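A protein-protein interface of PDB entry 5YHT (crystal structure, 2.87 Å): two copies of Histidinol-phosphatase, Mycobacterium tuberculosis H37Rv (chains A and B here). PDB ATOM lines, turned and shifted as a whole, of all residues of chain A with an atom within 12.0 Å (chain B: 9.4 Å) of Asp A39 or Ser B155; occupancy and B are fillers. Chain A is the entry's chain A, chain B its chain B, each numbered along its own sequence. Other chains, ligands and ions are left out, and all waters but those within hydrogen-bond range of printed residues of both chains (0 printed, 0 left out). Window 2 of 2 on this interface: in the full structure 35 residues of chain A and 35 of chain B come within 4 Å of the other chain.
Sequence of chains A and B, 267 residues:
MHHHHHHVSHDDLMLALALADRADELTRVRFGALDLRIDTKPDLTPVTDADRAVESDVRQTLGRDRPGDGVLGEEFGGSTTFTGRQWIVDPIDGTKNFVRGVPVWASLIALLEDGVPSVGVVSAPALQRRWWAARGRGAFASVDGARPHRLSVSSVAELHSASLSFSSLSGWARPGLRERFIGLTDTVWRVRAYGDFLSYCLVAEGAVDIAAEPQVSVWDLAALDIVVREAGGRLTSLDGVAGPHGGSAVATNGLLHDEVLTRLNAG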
ATOM      1  N   ASP A  35      16.387  -1.403 -21.296  1.00  0.00           N
ATOM      2  CA  ASP A  35      15.673  -0.686 -22.363  1.00  0.00           C
ATOM      3  C   ASP A  35      15.030   0.534 -21.734  1.00  0.00           C
ATOM      4  O   ASP A  35      14.075   0.412 -20.964  1.00  0.00           O
ATOM      5  CB  ASP A  35      14.621  -1.590 -23.041  1.00  0.00           C
ATOM      6  CG  ASP A  35      13.442  -0.803 -23.643  1.00  0.00           C
ATOM      7  OD1 ASP A  35      13.656   0.133 -24.453  1.00  0.00           O
ATOM      8  OD2 ASP A  35      12.290  -1.142 -23.295  1.00  0.00           O
ATOM      9  N   LEU A  36      15.557   1.707 -22.066  1.00  0.00           N
ATOM     10  CA  LEU A  36      15.205   2.917 -21.337  1.00  0.00           C
ATOM     11  C   LEU A  36      13.979   3.659 -21.892  1.00  0.00           C
ATOM     12  O   LEU A  36      13.434   4.546 -21.214  1.00  0.00           O
ATOM     13  CB  LEU A  36      16.436   3.812 -21.141  1.00  0.00           C
ATOM     14  CG  LEU A  36      17.354   3.346 -20.000  1.00  0.00           C
ATOM     15  N   ARG A  37      13.528   3.262 -23.092  1.00  0.00           N
ATOM     16  CA  ARG A  37      12.270   3.761 -23.673  1.00  0.00           C
ATOM     17  C   ARG A  37      11.119   3.493 -22.692  1.00  0.00           C
ATOM     18  O   ARG A  37      10.977   2.382 -22.170  1.00  0.00           O
ATOM     19  CB  ARG A  37      11.999   3.135 -25.048  1.00  0.00           C
ATOM     20  N   ILE A  38      10.345   4.538 -22.408  1.00  0.00           N
ATOM     21  CA  ILE A  38       9.275   4.487 -21.408  1.00  0.00           C
ATOM     22  C   ILE A  38       8.162   5.481 -21.784  1.00  0.00           C
ATOM     23  O   ILE A  38       8.435   6.491 -22.449  1.00  0.00           O
ATOM     24  CB  ILE A  38       9.826   4.799 -19.997  1.00  0.00           C
ATOM     25  CG1 ILE A  38       8.962   4.163 -18.909  1.00  0.00           C
ATOM     26  CD1 ILE A  38       9.120   4.844 -17.577  1.00  0.00           C
ATOM     27  N   ASP A  39       6.923   5.185 -21.370  1.00  0.00           N
ATOM     28  CA  ASP A  39       5.758   6.044 -21.648  1.00  0.00           C
ATOM     29  C   ASP A  39       4.681   6.060 -20.545  1.00  0.00           C
ATOM     30  O   ASP A  39       3.670   6.772 -20.656  1.00  0.00           O
ATOM     31  CB  ASP A  39       5.133   5.672 -22.996  1.00  0.00           C
ATOM     32  CG  ASP A  39       4.389   4.355 -22.948  1.00  0.00           C
ATOM     33  OD1 ASP A  39       5.021   3.311 -22.678  1.00  0.00           O
ATOM     34  OD2 ASP A  39       3.165   4.370 -23.172  1.00  0.00           O
ATOM     35  N   THR A  40       4.911   5.267 -19.500  1.00  0.00           N
ATOM     36  CA  THR A  40       4.053   5.202 -18.313  1.00  0.00           C
ATOM     37  C   THR A  40       4.950   4.928 -17.088  1.00  0.00           C
ATOM     38  O   THR A  40       6.179   5.005 -17.203  1.00  0.00           O
ATOM     39  CB  THR A  40       2.962   4.119 -18.471  1.00  0.00           C
ATOM     40  N   LYS A  41       4.359   4.633 -15.924  1.00  0.00           N
ATOM     41  CA  LYS A  41       5.136   4.187 -14.761  1.00  0.00           C
ATOM     42  C   LYS A  41       5.994   3.001 -15.202  1.00  0.00           C
ATOM     43  O   LYS A  41       5.526   2.183 -15.997  1.00  0.00           O
ATOM     44  CB  LYS A  41       4.226   3.811 -13.586  1.00  0.00           C
ATOM     45  CG  LYS A  41       3.605   5.005 -12.863  1.00  0.00           C
ATOM     46  CD  LYS A  41       2.683   4.612 -11.709  1.00  0.00           C
ATOM     47  CE  LYS A  41       3.397   3.762 -10.650  1.00  0.00           C
ATOM     48  NZ  LYS A  41       2.696   3.615  -9.336  1.00  0.00           N
ATOM     49  N   PRO A  42       7.263   2.928 -14.742  1.00  0.00           N
ATOM     50  CA  PRO A  42       8.171   1.941 -15.339  1.00  0.00           C
ATOM     51  C   PRO A  42       7.920   0.496 -14.900  1.00  0.00           C
ATOM     52  O   PRO A  42       7.464   0.244 -13.773  1.00  0.00           O
ATOM     53  CB  PRO A  42       9.563   2.395 -14.879  1.00  0.00           C
ATOM     54  CG  PRO A  42       9.356   3.579 -13.997  1.00  0.00           C
ATOM     55  CD  PRO A  42       7.908   3.649 -13.633  1.00  0.00           C
ATOM     56  N   ASP A  43       8.206  -0.425 -15.821  1.00  0.00           N
ATOM     57  CA  ASP A  43       8.260  -1.858 -15.553  1.00  0.00           C
ATOM     58  C   ASP A  43       9.401  -2.109 -14.553  1.00  0.00           C
ATOM     59  O   ASP A  43      10.584  -2.136 -14.930  1.00  0.00           O
ATOM     60  CB  ASP A  43       8.492  -2.619 -16.877  1.00  0.00           C
ATOM     61  CG  ASP A  43       8.027  -4.082 -16.837  1.00  0.00           C
ATOM     62  OD1 ASP A  43       7.782  -4.638 -15.742  1.00  0.00           O
ATOM     63  OD2 ASP A  43       7.921  -4.681 -17.933  1.00  0.00           O
ATOM     64  N   LEU A  44       9.029  -2.239 -13.276  1.00  0.00           N
ATOM     65  CA  LEU A  44       9.966  -2.572 -12.202  1.00  0.00           C
ATOM     66  C   LEU A  44      10.531  -3.993 -12.334  1.00  0.00           C
ATOM     67  O   LEU A  44      11.539  -4.307 -11.703  1.00  0.00           O
ATOM     68  CB  LEU A  44       9.314  -2.378 -10.829  1.00  0.00           C
ATOM     69  CG  LEU A  44       9.238  -0.957 -10.270  1.00  0.00           C
ATOM     70  N   VAL A  99      15.763   1.914 -12.940  1.00  0.00           N
ATOM     71  CA  VAL A  99      14.808   1.651 -14.024  1.00  0.00           C
ATOM     72  C   VAL A  99      14.609   2.816 -15.023  1.00  0.00           C
ATOM     73  O   VAL A  99      14.267   2.586 -16.192  1.00  0.00           O
ATOM     74  CB  VAL A  99      13.460   1.142 -13.449  1.00  0.00           C
ATOM     75  CG1 VAL A  99      12.703   2.242 -12.698  1.00  0.00           C
ATOM     76  CG2 VAL A  99      12.594   0.482 -14.520  1.00  0.00           C
ATOM     77  N   ARG A 100      14.835   4.052 -14.571  1.00  0.00           N
ATOM     78  CA  ARG A 100      14.774   5.222 -15.456  1.00  0.00           C
ATOM     79  C   ARG A 100      16.121   5.584 -16.123  1.00  0.00           C
ATOM     80  O   ARG A 100      16.174   6.475 -16.979  1.00  0.00           O
ATOM     81  CB  ARG A 100      14.160   6.429 -14.736  1.00  0.00           C
ATOM     82  CG  ARG A 100      12.649   6.354 -14.482  1.00  0.00           C
ATOM     83  CD  ARG A 100      11.800   6.280 -15.753  1.00  0.00           C
ATOM     84  NE  ARG A 100      12.024   7.379 -16.695  1.00  0.00           N
ATOM     85  CZ  ARG A 100      11.241   8.456 -16.799  1.00  0.00           C
ATOM     86  NH1 ARG A 100      10.169   8.578 -16.010  1.00  0.00           N
ATOM     87  NH2 ARG A 100      11.535   9.414 -17.688  1.00  0.00           N
ATOM     88  N   GLY A 101      17.194   4.880 -15.769  1.00  0.00           N
ATOM     89  CA  GLY A 101      18.534   5.208 -16.277  1.00  0.00           C
ATOM     90  C   GLY A 101      19.313   6.239 -15.456  1.00  0.00           C
ATOM     91  O   GLY A 101      20.402   6.639 -15.833  1.00  0.00           O
ATOM     92  N   SER B 152      17.320  11.349 -26.520  1.00  0.00           N
ATOM     93  CA  SER B 152      15.921  11.595 -26.784  1.00  0.00           C
ATOM     94  C   SER B 152      15.153  11.700 -25.486  1.00  0.00           C
ATOM     95  O   SER B 152      15.379  10.933 -24.547  1.00  0.00           O
ATOM     96  CB  SER B 152      15.317  10.494 -27.665  1.00  0.00           C
ATOM     97  N   VAL B 153      14.227  12.648 -25.439  1.00  0.00           N
ATOM     98  CA  VAL B 153      13.341  12.797 -24.285  1.00  0.00           C
ATOM     99  C   VAL B 153      12.451  11.562 -24.127  1.00  0.00           C
ATOM    100  O   VAL B 153      12.333  10.757 -25.055  1.00  0.00           O
ATOM    101  CB  VAL B 153      12.509  14.091 -24.377  1.00  0.00           C
ATOM    102  CG1 VAL B 153      13.427  15.265 -24.656  1.00  0.00           C
ATOM    103  CG2 VAL B 153      11.455  13.986 -25.459  1.00  0.00           C
ATOM    104  N   SER B 154      11.843  11.410 -22.951  1.00  0.00           N
ATOM    105  CA  SER B 154      10.997  10.252 -22.664  1.00  0.00           C
ATOM    106  C   SER B 154       9.674  10.355 -23.405  1.00  0.00           C
ATOM    107  O   SER B 154       9.357  11.409 -23.978  1.00  0.00           O
ATOM    108  CB  SER B 154      10.717  10.174 -21.174  1.00  0.00           C
ATOM    109  OG  SER B 154       9.674  11.069 -20.843  1.00  0.00           O
ATOM    110  N   SER B 155       8.892   9.273 -23.364  1.00  0.00           N
ATOM    111  CA  SER B 155       7.552   9.260 -23.965  1.00  0.00           C
ATOM    112  C   SER B 155       6.421   9.281 -22.948  1.00  0.00           C
ATOM    113  O   SER B 155       5.279   8.920 -23.255  1.00  0.00           O
ATOM    114  CB  SER B 155       7.409   8.097 -24.931  1.00  0.00           C
ATOM    115  OG  SER B 155       8.013   8.475 -26.151  1.00  0.00           O
ATOM    116  N   VAL B 156       6.744   9.727 -21.737  1.00  0.00           N
ATOM    117  CA  VAL B 156       5.778   9.785 -20.661  1.00  0.00           C
ATOM    118  C   VAL B 156       4.756  10.871 -20.962  1.00  0.00           C
ATOM    119  O   VAL B 156       5.095  12.059 -21.082  1.00  0.00           O
ATOM    120  CB  VAL B 156       6.459  10.005 -19.311  1.00  0.00           C
ATOM    121  CG1 VAL B 156       5.424  10.123 -18.197  1.00  0.00           C
ATOM    122  CG2 VAL B 156       7.429   8.865 -19.032  1.00  0.00           C
ATOM    123  N   ALA B 157       3.505  10.434 -21.106  1.00  0.00           N
ATOM    124  CA  ALA B 157       2.415  11.321 -21.491  1.00  0.00           C
ATOM    125  C   ALA B 157       1.544  11.749 -20.321  1.00  0.00           C
ATOM    126  O   ALA B 157       0.920  12.801 -20.386  1.00  0.00           O
ATOM    127  CB  ALA B 157       1.573  10.671 -22.563  1.00  0.00           C
ATOM    128  N   GLU B 158       1.503  10.949 -19.256  1.00  0.00           N
ATOM    129  CA  GLU B 158       0.634  11.244 -18.112  1.00  0.00           C
ATOM    130  C   GLU B 158       1.392  11.744 -16.876  1.00  0.00           C
ATOM    131  O   GLU B 158       2.297  11.062 -16.393  1.00  0.00           O
ATOM    132  CB  GLU B 158      -0.222  10.020 -17.758  1.00  0.00           C
ATOM    133  N   LEU B 159       0.986  12.915 -16.364  1.00  0.00           N
ATOM    134  CA  LEU B 159       1.609  13.561 -15.204  1.00  0.00           C
ATOM    135  C   LEU B 159       1.787  12.600 -14.023  1.00  0.00           C
ATOM    136  O   LEU B 159       2.852  12.582 -13.408  1.00  0.00           O
ATOM    137  CB  LEU B 159       0.813  14.804 -14.787  1.00  0.00           C
ATOM    138  CG  LEU B 159       1.539  16.055 -14.293  1.00  0.00           C
ATOM    139  N   HIS B 160       0.771  11.775 -13.747  1.00  0.00           N
ATOM    140  CA  HIS B 160       0.782  10.798 -12.629  1.00  0.00           C
ATOM    141  C   HIS B 160       1.873   9.732 -12.770  1.00  0.00           C
ATOM    142  O   HIS B 160       2.162   9.012 -11.815  1.00  0.00           O
ATOM    143  CB  HIS B 160      -0.589  10.122 -12.482  1.00  0.00           C
ATOM    144  CG  HIS B 160      -1.693  10.846 -13.192  1.00  0.00           C
ATOM    145  ND1 HIS B 160      -2.068  10.542 -14.484  1.00  0.00           N
ATOM    146  CD2 HIS B 160      -2.466  11.893 -12.813  1.00  0.00           C
ATOM    147  CE1 HIS B 160      -3.043  11.351 -14.861  1.00  0.00           C
ATOM    148  NE2 HIS B 160      -3.303  12.181 -13.866  1.00  0.00           N
ATOM    149  N   SER B 161       2.480   9.660 -13.957  1.00  0.00           N
ATOM    150  CA  SER B 161       3.563   8.715 -14.261  1.00  0.00           C
ATOM    151  C   SER B 161       4.934   9.375 -14.450  1.00  0.00           C
ATOM    152  O   SER B 161       5.931   8.677 -14.717  1.00  0.00           O
ATOM    153  CB  SER B 161       3.218   7.919 -15.523  1.00  0.00           C
ATOM    154  OG  SER B 161       2.259   6.921 -15.240  1.00  0.00           O
ATOM    155  N   ALA B 162       4.979  10.706 -14.312  1.00  0.00           N
ATOM    156  CA  ALA B 162       6.185  11.506 -14.632  1.00  0.00           C
ATOM    157  C   ALA B 162       7.184  11.608 -13.484  1.00  0.00           C
ATOM    158  O   ALA B 162       6.788  11.637 -12.304  1.00  0.00           O
ATOM    159  CB  ALA B 162       5.803  12.889 -15.121  1.00  0.00           C
ATOM    160  N   VAL B 203      16.322  15.525 -18.196  1.00  0.00           N
ATOM    161  CA  VAL B 203      15.167  15.663 -19.080  1.00  0.00           C
ATOM    162  C   VAL B 203      15.585  15.328 -20.510  1.00  0.00           C
ATOM    163  O   VAL B 203      14.968  14.463 -21.147  1.00  0.00           O
ATOM    164  CB  VAL B 203      14.483  17.048 -18.956  1.00  0.00           C
ATOM    165  CG1 VAL B 203      13.671  17.398 -20.192  1.00  0.00           C
ATOM    166  CG2 VAL B 203      13.563  17.056 -17.742  1.00  0.00           C
ATOM    167  N   GLU B 205      18.075  13.601 -21.511  1.00  0.00           N
ATOM    168  CA  GLU B 205      18.422  12.188 -21.575  1.00  0.00           C
ATOM    169  C   GLU B 205      17.205  11.291 -21.575  1.00  0.00           C
ATOM    170  O   GLU B 205      17.303  10.134 -21.963  1.00  0.00           O
ATOM    171  CB  GLU B 205      19.314  11.806 -20.403  1.00  0.00           C
ATOM    172  CG  GLU B 205      20.788  12.068 -20.657  1.00  0.00           C
ATOM    173  CD  GLU B 205      21.683  11.643 -19.516  1.00  0.00           C
ATOM    174  OE1 GLU B 205      21.188  11.051 -18.526  1.00  0.00           O
ATOM    175  OE2 GLU B 205      22.897  11.916 -19.616  1.00  0.00           O
ATOM    176  N   GLY B 206      16.064  11.825 -21.147  1.00  0.00           N
ATOM    177  CA  GLY B 206      14.846  11.047 -21.028  1.00  0.00           C
ATOM    178  C   GLY B 206      14.731  10.285 -19.713  1.00  0.00           C
ATOM    179  O   GLY B 206      13.808   9.480 -19.537  1.00  0.00           O
ATOM    180  N   ALA B 207      15.642  10.547 -18.775  1.00  0.00           N
ATOM    181  CA  ALA B 207      15.664   9.851 -17.472  1.00  0.00           C
ATOM    182  C   ALA B 207      14.738  10.521 -16.455  1.00  0.00           C
ATOM    183  O   ALA B 207      14.396   9.960 -15.406  1.00  0.00           O
ATOM    184  CB  ALA B 207      17.086   9.801 -16.941  1.00  0.00           C
ATOM    185  N   VAL B 208      14.364  11.749 -16.785  1.00  0.00           N
ATOM    186  CA  VAL B 208      13.479  12.565 -15.989  1.00  0.00           C
ATOM    187  C   VAL B 208      12.531  13.149 -17.026  1.00  0.00           C
ATOM    188  O   VAL B 208      12.905  13.280 -18.214  1.00  0.00           O
ATOM    189  CB  VAL B 208      14.304  13.655 -15.252  1.00  0.00           C
ATOM    190  CG1 VAL B 208      13.436  14.735 -14.614  1.00  0.00           C
ATOM    191  CG2 VAL B 208      15.195  13.009 -14.204  1.00  0.00           C
ATOM    192  N   ASP B 209      11.315  13.477 -16.598  1.00  0.00           N
ATOM    193  CA  ASP B 209      10.309  14.032 -17.511  1.00  0.00           C
ATOM    194  C   ASP B 209      10.049  15.541 -17.348  1.00  0.00           C
ATOM    195  O   ASP B 209       9.603  16.198 -18.291  1.00  0.00           O
ATOM    196  CB  ASP B 209       9.010  13.247 -17.402  1.00  0.00           C
ATOM    197  CG  ASP B 209       9.247  11.741 -17.334  1.00  0.00           C
ATOM    198  OD1 ASP B 209       9.835  11.204 -18.303  1.00  0.00           O
ATOM    199  OD2 ASP B 209       8.858  11.097 -16.306  1.00  0.00           O
ATOM    200  N   ALA B 231      17.185  17.226 -28.214  1.00  0.00           N
ATOM    201  CA  ALA B 231      16.797  15.935 -27.650  1.00  0.00           C
ATOM    202  C   ALA B 231      15.317  15.655 -27.870  1.00  0.00           C
ATOM    203  O   ALA B 231      14.836  14.541 -27.627  1.00  0.00           O
ATOM    204  CB  ALA B 231      17.134  15.879 -26.174  1.00  0.00           C
ATOM    205  N   GLY B 232      14.597  16.679 -28.324  1.00  0.00           N
ATOM    206  CA  GLY B 232      13.168  16.553 -28.614  1.00  0.00           C
ATOM    207  C   GLY B 232      12.224  17.085 -27.551  1.00  0.00           C
ATOM    208  O   GLY B 232      11.027  16.816 -27.591  1.00  0.00           O
ATOM    209  N   THR B 252      10.616  19.996 -20.292  1.00  0.00           N
ATOM    210  CA  THR B 252       9.876  18.724 -20.293  1.00  0.00           C
ATOM    211  C   THR B 252      10.182  17.922 -21.552  1.00  0.00           C
ATOM    212  O   THR B 252      10.913  18.393 -22.429  1.00  0.00           O
ATOM    213  CB  THR B 252       8.351  18.938 -20.268  1.00  0.00           C
ATOM    214  OG1 THR B 252       7.955  19.644 -21.455  1.00  0.00           O
ATOM    215  CG2 THR B 252       7.911  19.698 -19.025  1.00  0.00           C
ATOM    216  N   ASN B 253       9.582  16.734 -21.654  1.00  0.00           N
ATOM    217  CA  ASN B 253       9.628  15.932 -22.879  1.00  0.00           C
ATOM    218  C   ASN B 253       8.669  16.441 -23.962  1.00  0.00           C
ATOM    219  O   ASN B 253       8.389  15.736 -24.926  1.00  0.00           O
ATOM    220  CB  ASN B 253       9.348  14.445 -22.576  1.00  0.00           C
ATOM    221  CG  ASN B 253       7.983  14.208 -21.947  1.00  0.00           C
ATOM    222  OD1 ASN B 253       7.172  15.128 -21.789  1.00  0.00           O
ATOM    223  ND2 ASN B 253       7.730  12.964 -21.566  1.00  0.00           N
ATOM    224  N   GLY B 254       8.140  17.647 -23.793  1.00  0.00           N
ATOM    225  CA  GLY B 254       7.167  18.193 -24.744  1.00  0.00           C
ATOM    226  C   GLY B 254       5.742  17.756 -24.457  1.00  0.00           C
ATOM    227  O   GLY B 254       4.861  18.601 -24.257  1.00  0.00           O
ATOM    228  N   LEU B 255       5.521  16.440 -24.417  1.00  0.00           N
ATOM    229  CA  LEU B 255       4.181  15.871 -24.211  1.00  0.00           C
ATOM    230  C   LEU B 255       3.548  16.387 -22.906  1.00  0.00           C
ATOM    231  O   LEU B 255       2.343  16.661 -22.856  1.00  0.00           O
ATOM    232  CB  LEU B 255       4.211  14.327 -24.257  1.00  0.00           C
ATOM    233  CG  LEU B 255       4.830  13.592 -25.457  1.00  0.00           C
ATOM    234  N   LEU B 256       4.378  16.567 -21.881  1.00  0.00           N
ATOM    235  CA  LEU B 256       3.920  16.983 -20.567  1.00  0.00           C
ATOM    236  C   LEU B 256       3.890  18.495 -20.386  1.00  0.00           C
ATOM    237  O   LEU B 256       3.391  18.986 -19.372  1.00  0.00           O
ATOM    238  CB  LEU B 256       4.810  16.371 -19.510  1.00  0.00           C
ATOM    239  CG  LEU B 256       4.472  14.951 -19.123  1.00  0.00           C
ATOM    240  CD1 LEU B 256       5.746  14.270 -18.661  1.00  0.00           C
ATOM    241  CD2 LEU B 256       3.434  14.965 -18.014  1.00  0.00           C
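Along chain A the printed residues that touch a printed residue of chain B span positions 38 to 100. Of the 24 printed residues of chain B, 9 touch a printed residue of chain A. Printed residues of chain B that touch a printed residue of chain A: Ser B154, Ser B155, Val B156, Ala B157, Ser B161, Gly B206, Ala B207, Val B208 and Asp B209. Among the printed residues, 12 pairs touch across the chains.
N of Val B156 sits at hydrogen-bond distance from OG of Ser B154 (3.3 Å). OG of Ser B154 sits at hydrogen-bond distance from OD1 of Asp B209, 2.5 Å away. OG of Ser B154 sits at hydrogen-bond distance from ND2 of Asn B253, 2.8 Å away. The side-chain amide nitrogen (ND2) of Asn B253 sits at hydrogen-bond distance from the backbone carbonyl oxygen (O) of Val B156 (2.8 Å). The backbone carbonyl oxygen of Asp B209 lies within hydrogen-bond range of the backbone NH of Asn B253.
Val B156 touches Ile A38. Asp A39 touches Ser B155 (CB to O, 3.3 Å). Asp A39 touches Val B156 (O to CA, 3.7 Å). Asp A39 touches Ala B157 (O to N, 3.7 Å). C of Thr A40 touches CB of Ser B161 (3.8 Å). NH2 of Arg A100 touches CB of Ser B154 (3.7 Å). Arg A100 touches Ala B207. NH2 of Arg A100 touches N of Val B208 (3.8 Å).
The backbone NH (N) of Ser B155 sits at hydrogen-bond distance from the backbone carbonyl oxygen (O) of Ile A38, 3.0 Å away. The backbone NH (N) of Lys A41 sits at hydrogen-bond distance from the side-chain hydroxyl (OG) of Ser B161 (3.2 Å). The guanidinium group (NH2) of Arg A100 lies within hydrogen-bond range of the backbone carbonyl oxygen (O) of Gly B206. The guanidinium group (NH2) of Arg A100 lies within salt-bridge range of the side-chain carboxylate (OD1) of Asp B209 (2.5 Å).
Asp A39 touches just these residues of chain B: Ser B155, Val B156 and Ala B157. Of chain A, only Ile A38 and Asp A39 come within 4 Å of Ser B155. Of chain B, only Ser B155 (3.0 Å) and Val B156 (3.7 Å) come within 4 Å of Ile A38. Val B153 touches none of the printed residues of chain A. Ser B154 touches one residue of chain A. Of chain A, only Asp A39 (3.7 Å) comes within 4 Å of Ala B157. Ser B161 touches two residues of chain A. Printed residues of chain A within 4 Å of Gly B206: Arg A100. No residue of chain A comes within 4 Å of Asn B253. Of the printed residues of chain A, Ala B207 touches Arg A100. Printed residues of chain A within 4 Å of Val B208: Arg A100. Of the printed residues of chain B, Arg A100 touches Ser B154, Gly B206, Ala B207, Val B208 and Asp B209. Of the printed residues of chain A, Asp B209 touches Arg A100 (2.5 Å). Ser B152 touches none of the printed residues of chain A. Gly B254 touches none of the printed residues of chain A. The nearest residue of chain A that does not touch Ser B155 is Thr A40 (5.3 Å). The nearest printed residue of chain A that does not touch Ala B207 is Gly A101 (4.5 Å).
No position is printed for both chains. Of the 12 pairs that touch across the chains among the printed residues, none has its exchanged pair printed and touching as well.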
